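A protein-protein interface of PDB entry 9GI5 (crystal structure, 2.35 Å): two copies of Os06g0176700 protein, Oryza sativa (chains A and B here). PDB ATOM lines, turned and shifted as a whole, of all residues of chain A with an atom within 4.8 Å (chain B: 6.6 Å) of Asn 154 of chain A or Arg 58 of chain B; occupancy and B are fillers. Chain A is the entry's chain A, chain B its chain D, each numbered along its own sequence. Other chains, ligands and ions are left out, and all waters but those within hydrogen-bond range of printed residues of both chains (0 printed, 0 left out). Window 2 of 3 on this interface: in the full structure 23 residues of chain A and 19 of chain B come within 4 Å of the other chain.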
ATOM      1  N   GLU A 123      -5.758   5.496 -18.231  1.00  0.00           N
ATOM      2  CA  GLU A 123      -6.219   6.817 -17.836  1.00  0.00           C
ATOM      3  C   GLU A 123      -5.224   7.487 -16.894  1.00  0.00           C
ATOM      4  O   GLU A 123      -4.815   6.904 -15.886  1.00  0.00           O
ATOM      5  CB  GLU A 123      -7.588   6.708 -17.174  1.00  0.00           C
ATOM      6  CG  GLU A 123      -8.166   8.049 -16.829  1.00  0.00           C
ATOM      7  CD  GLU A 123      -9.671   8.017 -16.664  1.00  0.00           C
ATOM      8  OE1 GLU A 123     -10.195   7.038 -16.103  1.00  0.00           O
ATOM      9  OE2 GLU A 123     -10.335   8.966 -17.123  1.00  0.00           O
ATOM     10  N   GLU A 151     -20.383   6.428 -16.933  1.00  0.00           N
ATOM     11  CA  GLU A 151     -20.257   5.308 -16.004  1.00  0.00           C
ATOM     12  C   GLU A 151     -18.811   4.834 -15.878  1.00  0.00           C
ATOM     13  O   GLU A 151     -18.394   4.398 -14.797  1.00  0.00           O
ATOM     14  CB  GLU A 151     -21.159   4.151 -16.444  1.00  0.00           C
ATOM     15  CG  GLU A 151     -22.650   4.487 -16.504  1.00  0.00           C
ATOM     16  CD  GLU A 151     -23.089   5.040 -17.858  1.00  0.00           C
ATOM     17  OE1 GLU A 151     -22.251   5.649 -18.563  1.00  0.00           O
ATOM     18  OE2 GLU A 151     -24.274   4.865 -18.218  1.00  0.00           O
ATOM     19  N   GLU A 152     -18.031   4.902 -16.955  1.00  0.00           N
ATOM     20  CA  GLU A 152     -16.630   4.506 -16.897  1.00  0.00           C
ATOM     21  C   GLU A 152     -15.702   5.667 -16.558  1.00  0.00           C
ATOM     22  O   GLU A 152     -14.479   5.489 -16.542  1.00  0.00           O
ATOM     23  CB  GLU A 152     -16.206   3.869 -18.223  1.00  0.00           C
ATOM     24  CG  GLU A 152     -16.979   2.605 -18.576  1.00  0.00           C
ATOM     25  CD  GLU A 152     -16.770   2.197 -20.014  1.00  0.00           C
ATOM     26  OE1 GLU A 152     -15.804   2.696 -20.622  1.00  0.00           O
ATOM     27  OE2 GLU A 152     -17.566   1.389 -20.536  1.00  0.00           O
ATOM     28  N   ARG A 153     -16.251   6.846 -16.297  1.00  0.00           N
ATOM     29  CA  ARG A 153     -15.435   7.994 -15.937  1.00  0.00           C
ATOM     30  C   ARG A 153     -14.881   7.822 -14.524  1.00  0.00           C
ATOM     31  O   ARG A 153     -15.589   7.379 -13.616  1.00  0.00           O
ATOM     32  CB  ARG A 153     -16.273   9.265 -16.041  1.00  0.00           C
ATOM     33  CG  ARG A 153     -15.675  10.485 -15.375  1.00  0.00           C
ATOM     34  CD  ARG A 153     -16.589  11.688 -15.583  1.00  0.00           C
ATOM     35  NE  ARG A 153     -16.928  11.926 -16.984  1.00  0.00           N
ATOM     36  CZ  ARG A 153     -17.371  13.087 -17.454  1.00  0.00           C
ATOM     37  NH1 ARG A 153     -17.607  14.112 -16.649  1.00  0.00           N
ATOM     38  NH2 ARG A 153     -17.574  13.227 -18.761  1.00  0.00           N
ATOM     39  N   ASN A 154     -13.598   8.149 -14.349  1.00  0.00           N
ATOM     40  CA  ASN A 154     -12.920   8.077 -13.054  1.00  0.00           C
ATOM     41  C   ASN A 154     -12.392   9.476 -12.728  1.00  0.00           C
ATOM     42  O   ASN A 154     -11.268   9.833 -13.087  1.00  0.00           O
ATOM     43  CB  ASN A 154     -11.797   7.020 -13.061  1.00  0.00           C
ATOM     44  CG  ASN A 154     -11.168   6.818 -11.682  1.00  0.00           C
ATOM     45  OD1 ASN A 154     -11.532   7.490 -10.710  1.00  0.00           O
ATOM     46  ND2 ASN A 154     -10.245   5.863 -11.586  1.00  0.00           N
ATOM     47  N   LEU A 155     -13.213  10.259 -12.025  1.00  0.00           N
ATOM     48  CA  LEU A 155     -12.883  11.647 -11.722  1.00  0.00           C
ATOM     49  C   LEU A 155     -11.601  11.799 -10.909  1.00  0.00           C
ATOM     50  O   LEU A 155     -10.978  12.867 -10.951  1.00  0.00           O
ATOM     51  CB  LEU A 155     -14.036  12.296 -10.962  1.00  0.00           C
ATOM     52  CG  LEU A 155     -15.170  12.902 -11.786  1.00  0.00           C
ATOM     53  CD1 LEU A 155     -15.833  13.980 -10.957  1.00  0.00           C
ATOM     54  CD2 LEU A 155     -14.636  13.470 -13.079  1.00  0.00           C
ATOM     55  N   ALA A 156     -11.186  10.765 -10.178  1.00  0.00           N
ATOM     56  CA  ALA A 156     -10.006  10.908  -9.329  1.00  0.00           C
ATOM     57  C   ALA A 156      -8.734  11.146 -10.130  1.00  0.00           C
ATOM     58  O   ALA A 156      -7.739  11.601  -9.561  1.00  0.00           O
ATOM     59  CB  ALA A 156      -9.828   9.681  -8.436  1.00  0.00           C
ATOM     60  N   PHE A 157      -8.736  10.862 -11.428  1.00  0.00           N
ATOM     61  CA  PHE A 157      -7.573  11.120 -12.261  1.00  0.00           C
ATOM     62  C   PHE A 157      -7.713  12.393 -13.079  1.00  0.00           C
ATOM     63  O   PHE A 157      -6.791  12.738 -13.823  1.00  0.00           O
ATOM     64  CB  PHE A 157      -7.286   9.905 -13.156  1.00  0.00           C
ATOM     65  CG  PHE A 157      -6.790   8.719 -12.376  1.00  0.00           C
ATOM     66  CD1 PHE A 157      -5.437   8.585 -12.086  1.00  0.00           C
ATOM     67  CD2 PHE A 157      -7.675   7.777 -11.876  1.00  0.00           C
ATOM     68  CE1 PHE A 157      -4.973   7.521 -11.328  1.00  0.00           C
ATOM     69  CE2 PHE A 157      -7.221   6.708 -11.122  1.00  0.00           C
ATOM     70  CZ  PHE A 157      -5.866   6.577 -10.845  1.00  0.00           C
ATOM     71  N   TRP A 158      -8.829  13.107 -12.939  1.00  0.00           N
ATOM     72  CA  TRP A 158      -8.961  14.441 -13.518  1.00  0.00           C
ATOM     73  C   TRP A 158      -8.256  15.446 -12.610  1.00  0.00           C
ATOM     74  O   TRP A 158      -8.556  15.507 -11.414  1.00  0.00           O
ATOM     75  CB  TRP A 158     -10.437  14.817 -13.695  1.00  0.00           C
ATOM     76  CG  TRP A 158     -11.143  14.012 -14.765  1.00  0.00           C
ATOM     77  CD1 TRP A 158     -11.006  12.672 -15.004  1.00  0.00           C
ATOM     78  CD2 TRP A 158     -12.094  14.491 -15.729  1.00  0.00           C
ATOM     79  NE1 TRP A 158     -11.803  12.290 -16.051  1.00  0.00           N
ATOM     80  CE2 TRP A 158     -12.481  13.384 -16.519  1.00  0.00           C
ATOM     81  CE3 TRP A 158     -12.649  15.745 -16.007  1.00  0.00           C
ATOM     82  CZ2 TRP A 158     -13.403  13.494 -17.564  1.00  0.00           C
ATOM     83  CZ3 TRP A 158     -13.568  15.850 -17.044  1.00  0.00           C
ATOM     84  CH2 TRP A 158     -13.936  14.730 -17.807  1.00  0.00           C
ATOM     85  N   ASP B  55     -15.879  -4.929 -10.551  1.00  0.00           N
ATOM     86  CA  ASP B  55     -16.778  -3.999 -11.223  1.00  0.00           C
ATOM     87  C   ASP B  55     -16.305  -3.855 -12.665  1.00  0.00           C
ATOM     88  O   ASP B  55     -15.221  -3.321 -12.916  1.00  0.00           O
ATOM     89  CB  ASP B  55     -16.794  -2.655 -10.495  1.00  0.00           C
ATOM     90  CG  ASP B  55     -17.830  -1.694 -11.052  1.00  0.00           C
ATOM     91  OD1 ASP B  55     -18.034  -1.662 -12.284  1.00  0.00           O
ATOM     92  OD2 ASP B  55     -18.442  -0.960 -10.249  1.00  0.00           O
ATOM     93  N   LEU B  56     -17.117  -4.334 -13.613  1.00  0.00           N
ATOM     94  CA  LEU B  56     -16.703  -4.328 -15.014  1.00  0.00           C
ATOM     95  C   LEU B  56     -16.531  -2.910 -15.540  1.00  0.00           C
ATOM     96  O   LEU B  56     -15.589  -2.628 -16.288  1.00  0.00           O
ATOM     97  CB  LEU B  56     -17.711  -5.084 -15.880  1.00  0.00           C
ATOM     98  CG  LEU B  56     -17.279  -5.150 -17.347  1.00  0.00           C
ATOM     99  CD1 LEU B  56     -15.918  -5.820 -17.448  1.00  0.00           C
ATOM    100  CD2 LEU B  56     -18.303  -5.857 -18.220  1.00  0.00           C
ATOM    101  N   SER B  57     -17.432  -2.004 -15.161  1.00  0.00           N
ATOM    102  CA  SER B  57     -17.384  -0.643 -15.678  1.00  0.00           C
ATOM    103  C   SER B  57     -16.140   0.112 -15.232  1.00  0.00           C
ATOM    104  O   SER B  57     -15.855   1.184 -15.779  1.00  0.00           O
ATOM    105  CB  SER B  57     -18.633   0.125 -15.249  1.00  0.00           C
ATOM    106  OG  SER B  57     -18.447   0.688 -13.966  1.00  0.00           O
ATOM    107  N   ARG B  58     -15.398  -0.409 -14.258  1.00  0.00           N
ATOM    108  CA  ARG B  58     -14.193   0.248 -13.783  1.00  0.00           C
ATOM    109  C   ARG B  58     -12.944  -0.602 -13.990  1.00  0.00           C
ATOM    110  O   ARG B  58     -11.872  -0.239 -13.493  1.00  0.00           O
ATOM    111  CB  ARG B  58     -14.366   0.632 -12.308  1.00  0.00           C
ATOM    112  CG  ARG B  58     -15.606   1.504 -12.074  1.00  0.00           C
ATOM    113  CD  ARG B  58     -15.829   1.827 -10.606  1.00  0.00           C
ATOM    114  NE  ARG B  58     -14.769   2.665 -10.058  1.00  0.00           N
ATOM    115  CZ  ARG B  58     -14.594   3.946 -10.357  1.00  0.00           C
ATOM    116  NH1 ARG B  58     -15.394   4.579 -11.199  1.00  0.00           N
ATOM    117  NH2 ARG B  58     -13.581   4.607  -9.802  1.00  0.00           N
ATOM    118  N   LEU B  59     -13.044  -1.698 -14.749  1.00  0.00           N
ATOM    119  CA  LEU B  59     -11.937  -2.641 -14.875  1.00  0.00           C
ATOM    120  C   LEU B  59     -10.722  -2.041 -15.579  1.00  0.00           C
ATOM    121  O   LEU B  59      -9.608  -2.543 -15.396  1.00  0.00           O
ATOM    122  CB  LEU B  59     -12.409  -3.901 -15.610  1.00  0.00           C
ATOM    123  CG  LEU B  59     -11.461  -5.106 -15.647  1.00  0.00           C
ATOM    124  CD1 LEU B  59     -10.838  -5.339 -14.287  1.00  0.00           C
ATOM    125  CD2 LEU B  59     -12.185  -6.354 -16.125  1.00  0.00           C
ATOM    126  N   ALA B  60     -10.900  -0.981 -16.370  1.00  0.00           N
ATOM    127  CA  ALA B  60      -9.744  -0.318 -16.967  1.00  0.00           C
ATOM    128  C   ALA B  60      -8.817   0.276 -15.912  1.00  0.00           C
ATOM    129  O   ALA B  60      -7.614   0.410 -16.159  1.00  0.00           O
ATOM    130  CB  ALA B  60     -10.200   0.772 -17.939  1.00  0.00           C
ATOM    131  N   GLY B  61      -9.340   0.622 -14.740  1.00  0.00           N
ATOM    132  CA  GLY B  61      -8.496   1.150 -13.689  1.00  0.00           C
ATOM    133  C   GLY B  61      -7.627   0.077 -13.060  1.00  0.00           C
ATOM    134  O   GLY B  61      -7.997  -1.093 -12.977  1.00  0.00           O
ATOM    135  N   ALA B  62      -6.443   0.502 -12.606  1.00  0.00           N
ATOM    136  CA  ALA B  62      -5.509  -0.427 -11.980  1.00  0.00           C
ATOM    137  C   ALA B  62      -6.015  -0.910 -10.627  1.00  0.00           C
ATOM    138  O   ALA B  62      -5.641  -2.003 -10.185  1.00  0.00           O
ATOM    139  CB  ALA B  62      -4.139   0.232 -11.834  1.00  0.00           C
ATOM    140  N   ASP B  63      -6.847  -0.111  -9.950  1.00  0.00           N
ATOM    141  CA  ASP B  63      -7.453  -0.554  -8.696  1.00  0.00           C
ATOM    142  C   ASP B  63      -8.314  -1.792  -8.915  1.00  0.00           C
ATOM    143  O   ASP B  63      -8.179  -2.791  -8.200  1.00  0.00           O
ATOM    144  CB  ASP B  63      -8.294   0.570  -8.090  1.00  0.00           C
ATOM    145  CG  ASP B  63      -7.505   1.459  -7.151  1.00  0.00           C
ATOM    146  OD1 ASP B  63      -6.273   1.274  -7.035  1.00  0.00           O
ATOM    147  OD2 ASP B  63      -8.122   2.353  -6.534  1.00  0.00           O
ATOM    148  N   GLU B  64      -9.218  -1.735  -9.902  1.00  0.00           N
ATOM    149  CA  GLU B  64     -10.058  -2.889 -10.212  1.00  0.00           C
ATOM    150  C   GLU B  64      -9.240  -4.054 -10.745  1.00  0.00           C
ATOM    151  O   GLU B  64      -9.478  -5.207 -10.369  1.00  0.00           O
ATOM    152  CB  GLU B  64     -11.143  -2.514 -11.223  1.00  0.00           C
ATOM    153  CG  GLU B  64     -12.323  -1.828 -10.592  1.00  0.00           C
ATOM    154  CD  GLU B  64     -13.079  -2.728  -9.624  1.00  0.00           C
ATOM    155  OE1 GLU B  64     -13.887  -2.192  -8.842  1.00  0.00           O
ATOM    156  OE2 GLU B  64     -12.899  -3.965  -9.658  1.00  0.00           O
ATOM    157  N   ALA B  65      -8.283  -3.778 -11.634  1.00  0.00           N
ATOM    158  CA  ALA B  65      -7.470  -4.854 -12.184  1.00  0.00           C
ATOM    159  C   ALA B  65      -6.721  -5.598 -11.087  1.00  0.00           C
ATOM    160  O   ALA B  65      -6.454  -6.798 -11.220  1.00  0.00           O
ATOM    161  CB  ALA B  65      -6.500  -4.299 -13.226  1.00  0.00           C
ATOM    162  N   THR B  81     -19.994  -7.253 -11.314  1.00  0.00           N
ATOM    163  CA  THR B  81     -21.027  -6.251 -11.121  1.00  0.00           C
ATOM    164  C   THR B  81     -20.839  -5.141 -12.149  1.00  0.00           C
ATOM    165  O   THR B  81     -19.758  -4.978 -12.727  1.00  0.00           O
ATOM    166  CB  THR B  81     -21.010  -5.693  -9.686  1.00  0.00           C
ATOM    167  OG1 THR B  81     -22.266  -5.062  -9.404  1.00  0.00           O
ATOM    168  CG2 THR B  81     -19.872  -4.693  -9.491  1.00  0.00           C
ATOM    169  N   ASN B  82     -21.919  -4.399 -12.394  1.00  0.00           N
ATOM    170  CA  ASN B  82     -21.944  -3.361 -13.424  1.00  0.00           C
ATOM    171  C   ASN B  82     -21.440  -3.910 -14.757  1.00  0.00           C
ATOM    172  O   ASN B  82     -20.622  -3.301 -15.446  1.00  0.00           O
ATOM    173  CB  ASN B  82     -21.141  -2.134 -12.993  1.00  0.00           C
ATOM    174  CG  ASN B  82     -21.763  -1.423 -11.809  1.00  0.00           C
ATOM    175  OD1 ASN B  82     -21.211  -1.415 -10.709  1.00  0.00           O
ATOM    176  ND2 ASN B  82     -22.930  -0.830 -12.030  1.00  0.00           N
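Of chain B, only Arg 58 (3.7 Å) comes within 4 Å of Asn 154 of chain A.
Arg 58 of chain B touches just these residues of chain A: Arg 153 (3.7 Å) and Asn 154 (3.7 Å).
Of the printed residues of chain B, Glu 151 of chain A touches Ser 57.
Of the printed residues of chain B, Glu 152 of chain A touches Ser 57 (3.3 Å).
Printed residues of chain A within 4 Å of Ser 57 of chain B: Glu 151 and Glu 152.
Of the printed residues of chain B, Arg 153 of chain A touches Arg 58 (3.7 Å).
Asp 63 of chain B touches none of the printed residues of chain A.
Gly 61 of chain B touches none of the printed residues of chain A.
The nearest residue of chain A that does not touch Arg 58 of chain B is Glu 151 of chain A (4.7 Å).
Of the 13 printed residues of chain B, 2 touch a printed residue of chain A.
Printed residues of chain B that touch a printed residue of chain A: Ser 57 and Arg 58.
Among the printed residues, no Asp or Glu carboxylate lies within 4 Å of a Lys or Arg side-chain nitrogen of the other chain.
O of Glu 151 of chain A touches OG of Ser 57 of chain B, at 3.8 Å.
O of Ser 57 of chain B touches CG of Glu 152 of chain A, at 3.3 Å.
Arg 58 of chain B touches Arg 153 of chain A (NH1 to O, 3.7 Å).
Arg 58 of chain B touches Asn 154 of chain A (NH2 to OD1, 3.7 Å).
The side-chain amide oxygen of Asn 154 of chain A lies close to the backbone NH of Ala 156 of chain A (3.3 Å).
OD1 of Asp 55 of chain B sits at hydrogen-bond distance from OG of Ser 57 of chain B, 2.9 Å away.
N of Ser 57 of chain B sits at hydrogen-bond distance from O of Asn 82 of chain B (3.5 Å).
No position is printed for both chains.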
